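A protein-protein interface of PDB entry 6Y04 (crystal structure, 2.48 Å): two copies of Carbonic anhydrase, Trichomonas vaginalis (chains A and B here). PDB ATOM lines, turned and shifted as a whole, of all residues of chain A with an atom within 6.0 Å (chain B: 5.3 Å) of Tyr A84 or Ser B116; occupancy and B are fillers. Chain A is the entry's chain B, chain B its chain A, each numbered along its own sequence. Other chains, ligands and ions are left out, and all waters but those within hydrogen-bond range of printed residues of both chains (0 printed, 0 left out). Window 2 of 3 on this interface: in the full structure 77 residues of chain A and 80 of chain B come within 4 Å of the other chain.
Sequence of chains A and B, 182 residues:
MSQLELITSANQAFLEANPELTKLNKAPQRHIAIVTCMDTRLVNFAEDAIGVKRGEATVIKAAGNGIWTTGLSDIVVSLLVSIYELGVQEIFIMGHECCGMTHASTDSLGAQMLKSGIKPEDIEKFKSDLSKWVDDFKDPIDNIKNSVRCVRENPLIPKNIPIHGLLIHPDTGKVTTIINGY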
ATOM      1  N   LEU A  79      22.084  13.267  18.050  1.00  0.00           N
ATOM      2  CA  LEU A  79      21.843  11.900  18.482  1.00  0.00           C
ATOM      3  C   LEU A  79      20.496  11.784  19.202  1.00  0.00           C
ATOM      4  O   LEU A  79      19.797  10.783  19.038  1.00  0.00           O
ATOM      5  CB  LEU A  79      23.010  11.432  19.356  1.00  0.00           C
ATOM      6  CG  LEU A  79      24.334  11.264  18.613  1.00  0.00           C
ATOM      7  CD1 LEU A  79      25.480  11.001  19.576  1.00  0.00           C
ATOM      8  CD2 LEU A  79      24.240  10.165  17.575  1.00  0.00           C
ATOM      9  N   LEU A  80      20.123  12.811  19.981  1.00  0.00           N
ATOM     10  CA  LEU A  80      18.852  12.800  20.695  1.00  0.00           C
ATOM     11  C   LEU A  80      17.704  12.835  19.690  1.00  0.00           C
ATOM     12  O   LEU A  80      16.734  12.094  19.832  1.00  0.00           O
ATOM     13  CB  LEU A  80      18.770  13.990  21.659  1.00  0.00           C
ATOM     14  CG  LEU A  80      19.806  14.017  22.782  1.00  0.00           C
ATOM     15  CD1 LEU A  80      19.758  15.349  23.518  1.00  0.00           C
ATOM     16  CD2 LEU A  80      19.600  12.862  23.757  1.00  0.00           C
ATOM     17  N   VAL A  81      17.836  13.690  18.669  1.00  0.00           N
ATOM     18  CA  VAL A  81      16.846  13.786  17.611  1.00  0.00           C
ATOM     19  C   VAL A  81      16.780  12.453  16.868  1.00  0.00           C
ATOM     20  O   VAL A  81      15.696  11.961  16.572  1.00  0.00           O
ATOM     21  CB  VAL A  81      17.145  14.967  16.665  1.00  0.00           C
ATOM     22  CG1 VAL A  81      16.208  14.990  15.459  1.00  0.00           C
ATOM     23  CG2 VAL A  81      17.108  16.301  17.399  1.00  0.00           C
ATOM     24  N   SER A  82      17.945  11.869  16.575  1.00  0.00           N
ATOM     25  CA  SER A  82      17.990  10.603  15.859  1.00  0.00           C
ATOM     26  C   SER A  82      17.192   9.541  16.612  1.00  0.00           C
ATOM     27  O   SER A  82      16.394   8.823  16.010  1.00  0.00           O
ATOM     28  CB  SER A  82      19.410  10.151  15.614  1.00  0.00           C
ATOM     29  OG  SER A  82      20.045  10.988  14.667  1.00  0.00           O
ATOM     30  N   ILE A  83      17.409   9.454  17.931  1.00  0.00           N
ATOM     31  CA  ILE A  83      16.835   8.371  18.718  1.00  0.00           C
ATOM     32  C   ILE A  83      15.342   8.622  18.928  1.00  0.00           C
ATOM     33  O   ILE A  83      14.514   7.767  18.612  1.00  0.00           O
ATOM     34  CB  ILE A  83      17.579   8.177  20.057  1.00  0.00           C
ATOM     35  CG1 ILE A  83      19.051   7.806  19.857  1.00  0.00           C
ATOM     36  CG2 ILE A  83      16.861   7.156  20.928  1.00  0.00           C
ATOM     37  CD1 ILE A  83      19.913   8.073  21.071  1.00  0.00           C
ATOM     38  N   TYR A  84      15.022   9.811  19.445  1.00  0.00           N
ATOM     39  CA  TYR A  84      13.712  10.108  20.001  1.00  0.00           C
ATOM     40  C   TYR A  84      12.729  10.516  18.912  1.00  0.00           C
ATOM     41  O   TYR A  84      11.566  10.121  18.965  1.00  0.00           O
ATOM     42  CB  TYR A  84      13.823  11.162  21.101  1.00  0.00           C
ATOM     43  CG  TYR A  84      14.577  10.678  22.310  1.00  0.00           C
ATOM     44  CD1 TYR A  84      14.170   9.541  23.001  1.00  0.00           C
ATOM     45  CD2 TYR A  84      15.698  11.354  22.767  1.00  0.00           C
ATOM     46  CE1 TYR A  84      14.861   9.082  24.111  1.00  0.00           C
ATOM     47  CE2 TYR A  84      16.395  10.914  23.882  1.00  0.00           C
ATOM     48  CZ  TYR A  84      15.978   9.772  24.550  1.00  0.00           C
ATOM     49  OH  TYR A  84      16.671   9.341  25.643  1.00  0.00           O
ATOM     50  N   GLU A  85      13.203  11.285  17.926  1.00  0.00           N
ATOM     51  CA  GLU A  85      12.334  11.740  16.857  1.00  0.00           C
ATOM     52  C   GLU A  85      12.352  10.764  15.675  1.00  0.00           C
ATOM     53  O   GLU A  85      11.322  10.568  15.035  1.00  0.00           O
ATOM     54  CB  GLU A  85      12.656  13.190  16.483  1.00  0.00           C
ATOM     55  CG  GLU A  85      11.447  13.979  16.003  1.00  0.00           C
ATOM     56  CD  GLU A  85      10.454  14.496  17.042  1.00  0.00           C
ATOM     57  OE1 GLU A  85      10.691  14.322  18.272  1.00  0.00           O
ATOM     58  OE2 GLU A  85       9.430  15.085  16.614  1.00  0.00           O
ATOM     59  N   LEU A  86      13.497  10.128  15.393  1.00  0.00           N
ATOM     60  CA  LEU A  86      13.669   9.460  14.109  1.00  0.00           C
ATOM     61  C   LEU A  86      13.850   7.945  14.219  1.00  0.00           C
ATOM     62  O   LEU A  86      14.075   7.295  13.204  1.00  0.00           O
ATOM     63  CB  LEU A  86      14.831  10.105  13.348  1.00  0.00           C
ATOM     64  CG  LEU A  86      14.556  11.515  12.833  1.00  0.00           C
ATOM     65  CD1 LEU A  86      15.841  12.178  12.356  1.00  0.00           C
ATOM     66  CD2 LEU A  86      13.511  11.487  11.721  1.00  0.00           C
ATOM     67  N   GLY A  87      13.789   7.392  15.433  1.00  0.00           N
ATOM     68  CA  GLY A  87      13.726   5.950  15.622  1.00  0.00           C
ATOM     69  C   GLY A  87      15.082   5.238  15.572  1.00  0.00           C
ATOM     70  O   GLY A  87      15.127   4.031  15.375  1.00  0.00           O
ATOM     71  N   VAL A  88      16.188   5.960  15.773  1.00  0.00           N
ATOM     72  CA  VAL A  88      17.510   5.338  15.731  1.00  0.00           C
ATOM     73  C   VAL A  88      17.719   4.476  16.978  1.00  0.00           C
ATOM     74  O   VAL A  88      17.405   4.898  18.088  1.00  0.00           O
ATOM     75  CB  VAL A  88      18.635   6.380  15.565  1.00  0.00           C
ATOM     76  CG1 VAL A  88      19.988   5.831  15.998  1.00  0.00           C
ATOM     77  CG2 VAL A  88      18.707   6.908  14.142  1.00  0.00           C
ATOM     78  N   PRO A 155      23.154  11.323  30.437  1.00  0.00           N
ATOM     79  CA  PRO A 155      21.916  10.947  31.128  1.00  0.00           C
ATOM     80  C   PRO A 155      20.663  11.031  30.255  1.00  0.00           C
ATOM     81  O   PRO A 155      19.607  10.522  30.630  1.00  0.00           O
ATOM     82  CB  PRO A 155      21.831  11.959  32.280  1.00  0.00           C
ATOM     83  CG  PRO A 155      22.610  13.161  31.790  1.00  0.00           C
ATOM     84  CD  PRO A 155      23.712  12.596  30.919  1.00  0.00           C
ATOM     85  N   LEU A 156      20.789  11.672  29.087  1.00  0.00           N
ATOM     86  CA  LEU A 156      19.647  11.825  28.199  1.00  0.00           C
ATOM     87  C   LEU A 156      19.584  10.659  27.214  1.00  0.00           C
ATOM     88  O   LEU A 156      18.638  10.571  26.444  1.00  0.00           O
ATOM     89  CB  LEU A 156      19.751  13.156  27.447  1.00  0.00           C
ATOM     90  CG  LEU A 156      19.625  14.434  28.267  1.00  0.00           C
ATOM     91  CD1 LEU A 156      19.261  15.605  27.357  1.00  0.00           C
ATOM     92  CD2 LEU A 156      18.590  14.280  29.375  1.00  0.00           C
ATOM     93  N   ILE A 157      20.580   9.770  27.249  1.00  0.00           N
ATOM     94  CA  ILE A 157      20.682   8.704  26.268  1.00  0.00           C
ATOM     95  C   ILE A 157      20.370   7.358  26.920  1.00  0.00           C
ATOM     96  O   ILE A 157      21.038   6.957  27.873  1.00  0.00           O
ATOM     97  CB  ILE A 157      22.028   8.753  25.517  1.00  0.00           C
ATOM     98  CG1 ILE A 157      22.010   9.906  24.509  1.00  0.00           C
ATOM     99  CG2 ILE A 157      22.326   7.431  24.826  1.00  0.00           C
ATOM    100  CD1 ILE A 157      23.310  10.138  23.791  1.00  0.00           C
ATOM    101  N   PRO A 158      19.351   6.621  26.408  1.00  0.00           N
ATOM    102  CA  PRO A 158      18.879   5.383  27.034  1.00  0.00           C
ATOM    103  C   PRO A 158      19.989   4.342  27.076  1.00  0.00           C
ATOM    104  O   PRO A 158      20.866   4.337  26.219  1.00  0.00           O
ATOM    105  CB  PRO A 158      17.770   4.870  26.097  1.00  0.00           C
ATOM    106  CG  PRO A 158      17.352   6.088  25.296  1.00  0.00           C
ATOM    107  CD  PRO A 158      18.607   6.932  25.176  1.00  0.00           C
ATOM    108  N   ASN A 160      19.645   1.234  26.603  1.00  0.00           N
ATOM    109  CA  ASN A 160      19.376   0.147  25.673  1.00  0.00           C
ATOM    110  C   ASN A 160      19.764   0.520  24.237  1.00  0.00           C
ATOM    111  O   ASN A 160      19.433  -0.210  23.303  1.00  0.00           O
ATOM    112  CB  ASN A 160      17.922  -0.322  25.758  1.00  0.00           C
ATOM    113  CG  ASN A 160      16.934   0.678  25.192  1.00  0.00           C
ATOM    114  OD1 ASN A 160      17.071   1.890  25.371  1.00  0.00           O
ATOM    115  ND2 ASN A 160      15.925   0.169  24.503  1.00  0.00           N
ATOM    116  N   LEU B 109      10.481  15.953  22.666  1.00  0.00           N
ATOM    117  CA  LEU B 109      11.665  15.182  23.012  1.00  0.00           C
ATOM    118  C   LEU B 109      11.561  14.720  24.460  1.00  0.00           C
ATOM    119  O   LEU B 109      11.926  13.586  24.767  1.00  0.00           O
ATOM    120  CB  LEU B 109      12.930  16.009  22.774  1.00  0.00           C
ATOM    121  CG  LEU B 109      13.325  16.196  21.309  1.00  0.00           C
ATOM    122  CD1 LEU B 109      14.363  17.285  21.181  1.00  0.00           C
ATOM    123  CD2 LEU B 109      13.842  14.906  20.683  1.00  0.00           C
ATOM    124  N   GLN B 112       9.303  11.793  24.742  1.00  0.00           N
ATOM    125  CA  GLN B 112       9.960  10.600  24.223  1.00  0.00           C
ATOM    126  C   GLN B 112      10.951  10.045  25.246  1.00  0.00           C
ATOM    127  O   GLN B 112      11.049   8.833  25.438  1.00  0.00           O
ATOM    128  CB  GLN B 112      10.641  10.912  22.891  1.00  0.00           C
ATOM    129  CG  GLN B 112       9.660  11.080  21.735  1.00  0.00           C
ATOM    130  CD  GLN B 112       8.955   9.784  21.418  1.00  0.00           C
ATOM    131  OE1 GLN B 112       7.851   9.523  21.896  1.00  0.00           O
ATOM    132  NE2 GLN B 112       9.602   8.943  20.627  1.00  0.00           N
ATOM    133  N   MET B 113      11.653  10.955  25.929  1.00  0.00           N
ATOM    134  CA  MET B 113      12.662  10.587  26.907  1.00  0.00           C
ATOM    135  C   MET B 113      12.001   9.946  28.128  1.00  0.00           C
ATOM    136  O   MET B 113      12.507   8.961  28.666  1.00  0.00           O
ATOM    137  CB  MET B 113      13.490  11.808  27.318  1.00  0.00           C
ATOM    138  CG  MET B 113      14.197  12.470  26.139  1.00  0.00           C
ATOM    139  SD  MET B 113      15.396  13.773  26.537  1.00  0.00           S
ATOM    140  CE  MET B 113      14.323  15.088  27.099  1.00  0.00           C
ATOM    141  N   LEU B 114      10.861  10.506  28.549  1.00  0.00           N
ATOM    142  CA  LEU B 114      10.077   9.982  29.657  1.00  0.00           C
ATOM    143  C   LEU B 114       9.682   8.540  29.360  1.00  0.00           C
ATOM    144  O   LEU B 114       9.789   7.690  30.234  1.00  0.00           O
ATOM    145  CB  LEU B 114       8.839  10.862  29.868  1.00  0.00           C
ATOM    146  CG  LEU B 114       9.050  12.101  30.742  1.00  0.00           C
ATOM    147  CD1 LEU B 114       7.895  13.094  30.625  1.00  0.00           C
ATOM    148  CD2 LEU B 114       9.304  11.715  32.193  1.00  0.00           C
ATOM    149  N   LYS B 115       9.243   8.287  28.118  1.00  0.00           N
ATOM    150  CA  LYS B 115       8.889   6.952  27.648  1.00  0.00           C
ATOM    151  C   LYS B 115      10.071   6.000  27.822  1.00  0.00           C
ATOM    152  O   LYS B 115       9.883   4.814  28.090  1.00  0.00           O
ATOM    153  CB  LYS B 115       8.577   6.972  26.148  1.00  0.00           C
ATOM    154  CG  LYS B 115       7.147   6.745  25.696  1.00  0.00           C
ATOM    155  CD  LYS B 115       7.105   6.530  24.198  1.00  0.00           C
ATOM    156  CE  LYS B 115       5.789   6.945  23.571  1.00  0.00           C
ATOM    157  NZ  LYS B 115       5.640   6.412  22.195  1.00  0.00           N
ATOM    158  N   SER B 116      11.288   6.525  27.657  1.00  0.00           N
ATOM    159  CA  SER B 116      12.469   5.680  27.585  1.00  0.00           C
ATOM    160  C   SER B 116      13.110   5.524  28.964  1.00  0.00           C
ATOM    161  O   SER B 116      14.167   4.909  29.088  1.00  0.00           O
ATOM    162  CB  SER B 116      13.447   6.191  26.552  1.00  0.00           C
ATOM    163  OG  SER B 116      12.810   6.373  25.294  1.00  0.00           O
ATOM    164  N   GLY B 117      12.450   6.057  29.997  1.00  0.00           N
ATOM    165  CA  GLY B 117      12.875   5.839  31.368  1.00  0.00           C
ATOM    166  C   GLY B 117      13.991   6.797  31.771  1.00  0.00           C
ATOM    167  O   GLY B 117      14.749   6.516  32.697  1.00  0.00           O
ATOM    168  N   ILE B 118      14.084   7.929  31.062  1.00  0.00           N
ATOM    169  CA  ILE B 118      15.017   8.984  31.419  1.00  0.00           C
ATOM    170  C   ILE B 118      14.437   9.712  32.627  1.00  0.00           C
ATOM    171  O   ILE B 118      13.244  10.002  32.649  1.00  0.00           O
ATOM    172  CB  ILE B 118      15.248   9.937  30.226  1.00  0.00           C
ATOM    173  CG1 ILE B 118      15.792   9.220  28.983  1.00  0.00           C
ATOM    174  CG2 ILE B 118      16.090  11.145  30.622  1.00  0.00           C
ATOM    175  CD1 ILE B 118      17.121   8.518  29.168  1.00  0.00           C
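Of the 8 printed residues of chain B, 5 touch a printed residue of chain A. Printed residues of chain B that touch a printed residue of chain A: Leu B109, Gln B112, Met B113, Ser B116 and Ile B118. Along chain B the printed residues that touch a printed residue of chain A span positions 109 to 118. Among the printed residues, 7 pairs touch across the chains. Among the printed residues, no Asp or Glu carboxylate lies within 4 Å of a Lys or Arg side-chain nitrogen of the other chain.
The backbone carbonyl oxygen of Tyr A84 is in hydrogen-bond range of the side-chain amide nitrogen of Gln B112 (2.8 Å).
Leu A79 touches none of the printed residues of chain B. Of chain B, only Leu B109, Gln B112, Met B113, Ser B116 and Ile B118 come within 4 Å of Tyr A84. Printed residues of chain B within 4 Å of Pro A155: Ile B118. Of the printed residues of chain B, Leu A156 touches Ile B118 (3.7 Å). Of the printed residues of chain A, Leu B109 touches Tyr A84. Of the printed residues of chain A, Gln B112 touches Tyr A84. Lys B115 touches none of the printed residues of chain A. Ser B116 touches just one residue of chain A: Tyr A84 (3.6 Å). Of the printed residues of chain A, Ile B118 touches Tyr A84 (3.5 Å), Pro A155 (3.5 Å) and Leu A156 (3.7 Å). The nearest printed residue of chain B that does not touch Tyr A84 is Leu B114 (6.1 Å).
No position is printed for both chains. Of the 7 pairs that touch across the chains among the printed residues, none has its exchanged pair printed and touching as well.
CD2 of Leu B109 touches CB of Tyr A84, at 3.8 Å. Tyr A84 touches Met B113. Tyr A84 touches Ser B116. OH of Tyr A84 touches CG1 of Ile B118, at 3.5 Å. Ile B118 touches Pro A155. O of Leu A156 touches CD1 of Ile B118, at 3.7 Å.
The side-chain hydroxyl of Tyr A84 is in hydrogen-bond range of the backbone carbonyl oxygen of Leu A156 (2.5 Å). The backbone carbonyl oxygen of Gln B112 is in hydrogen-bond range of the side-chain hydroxyl of Ser B116 (3.0 Å). O of Met B113 lies within hydrogen-bond range of N of Ile B118.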
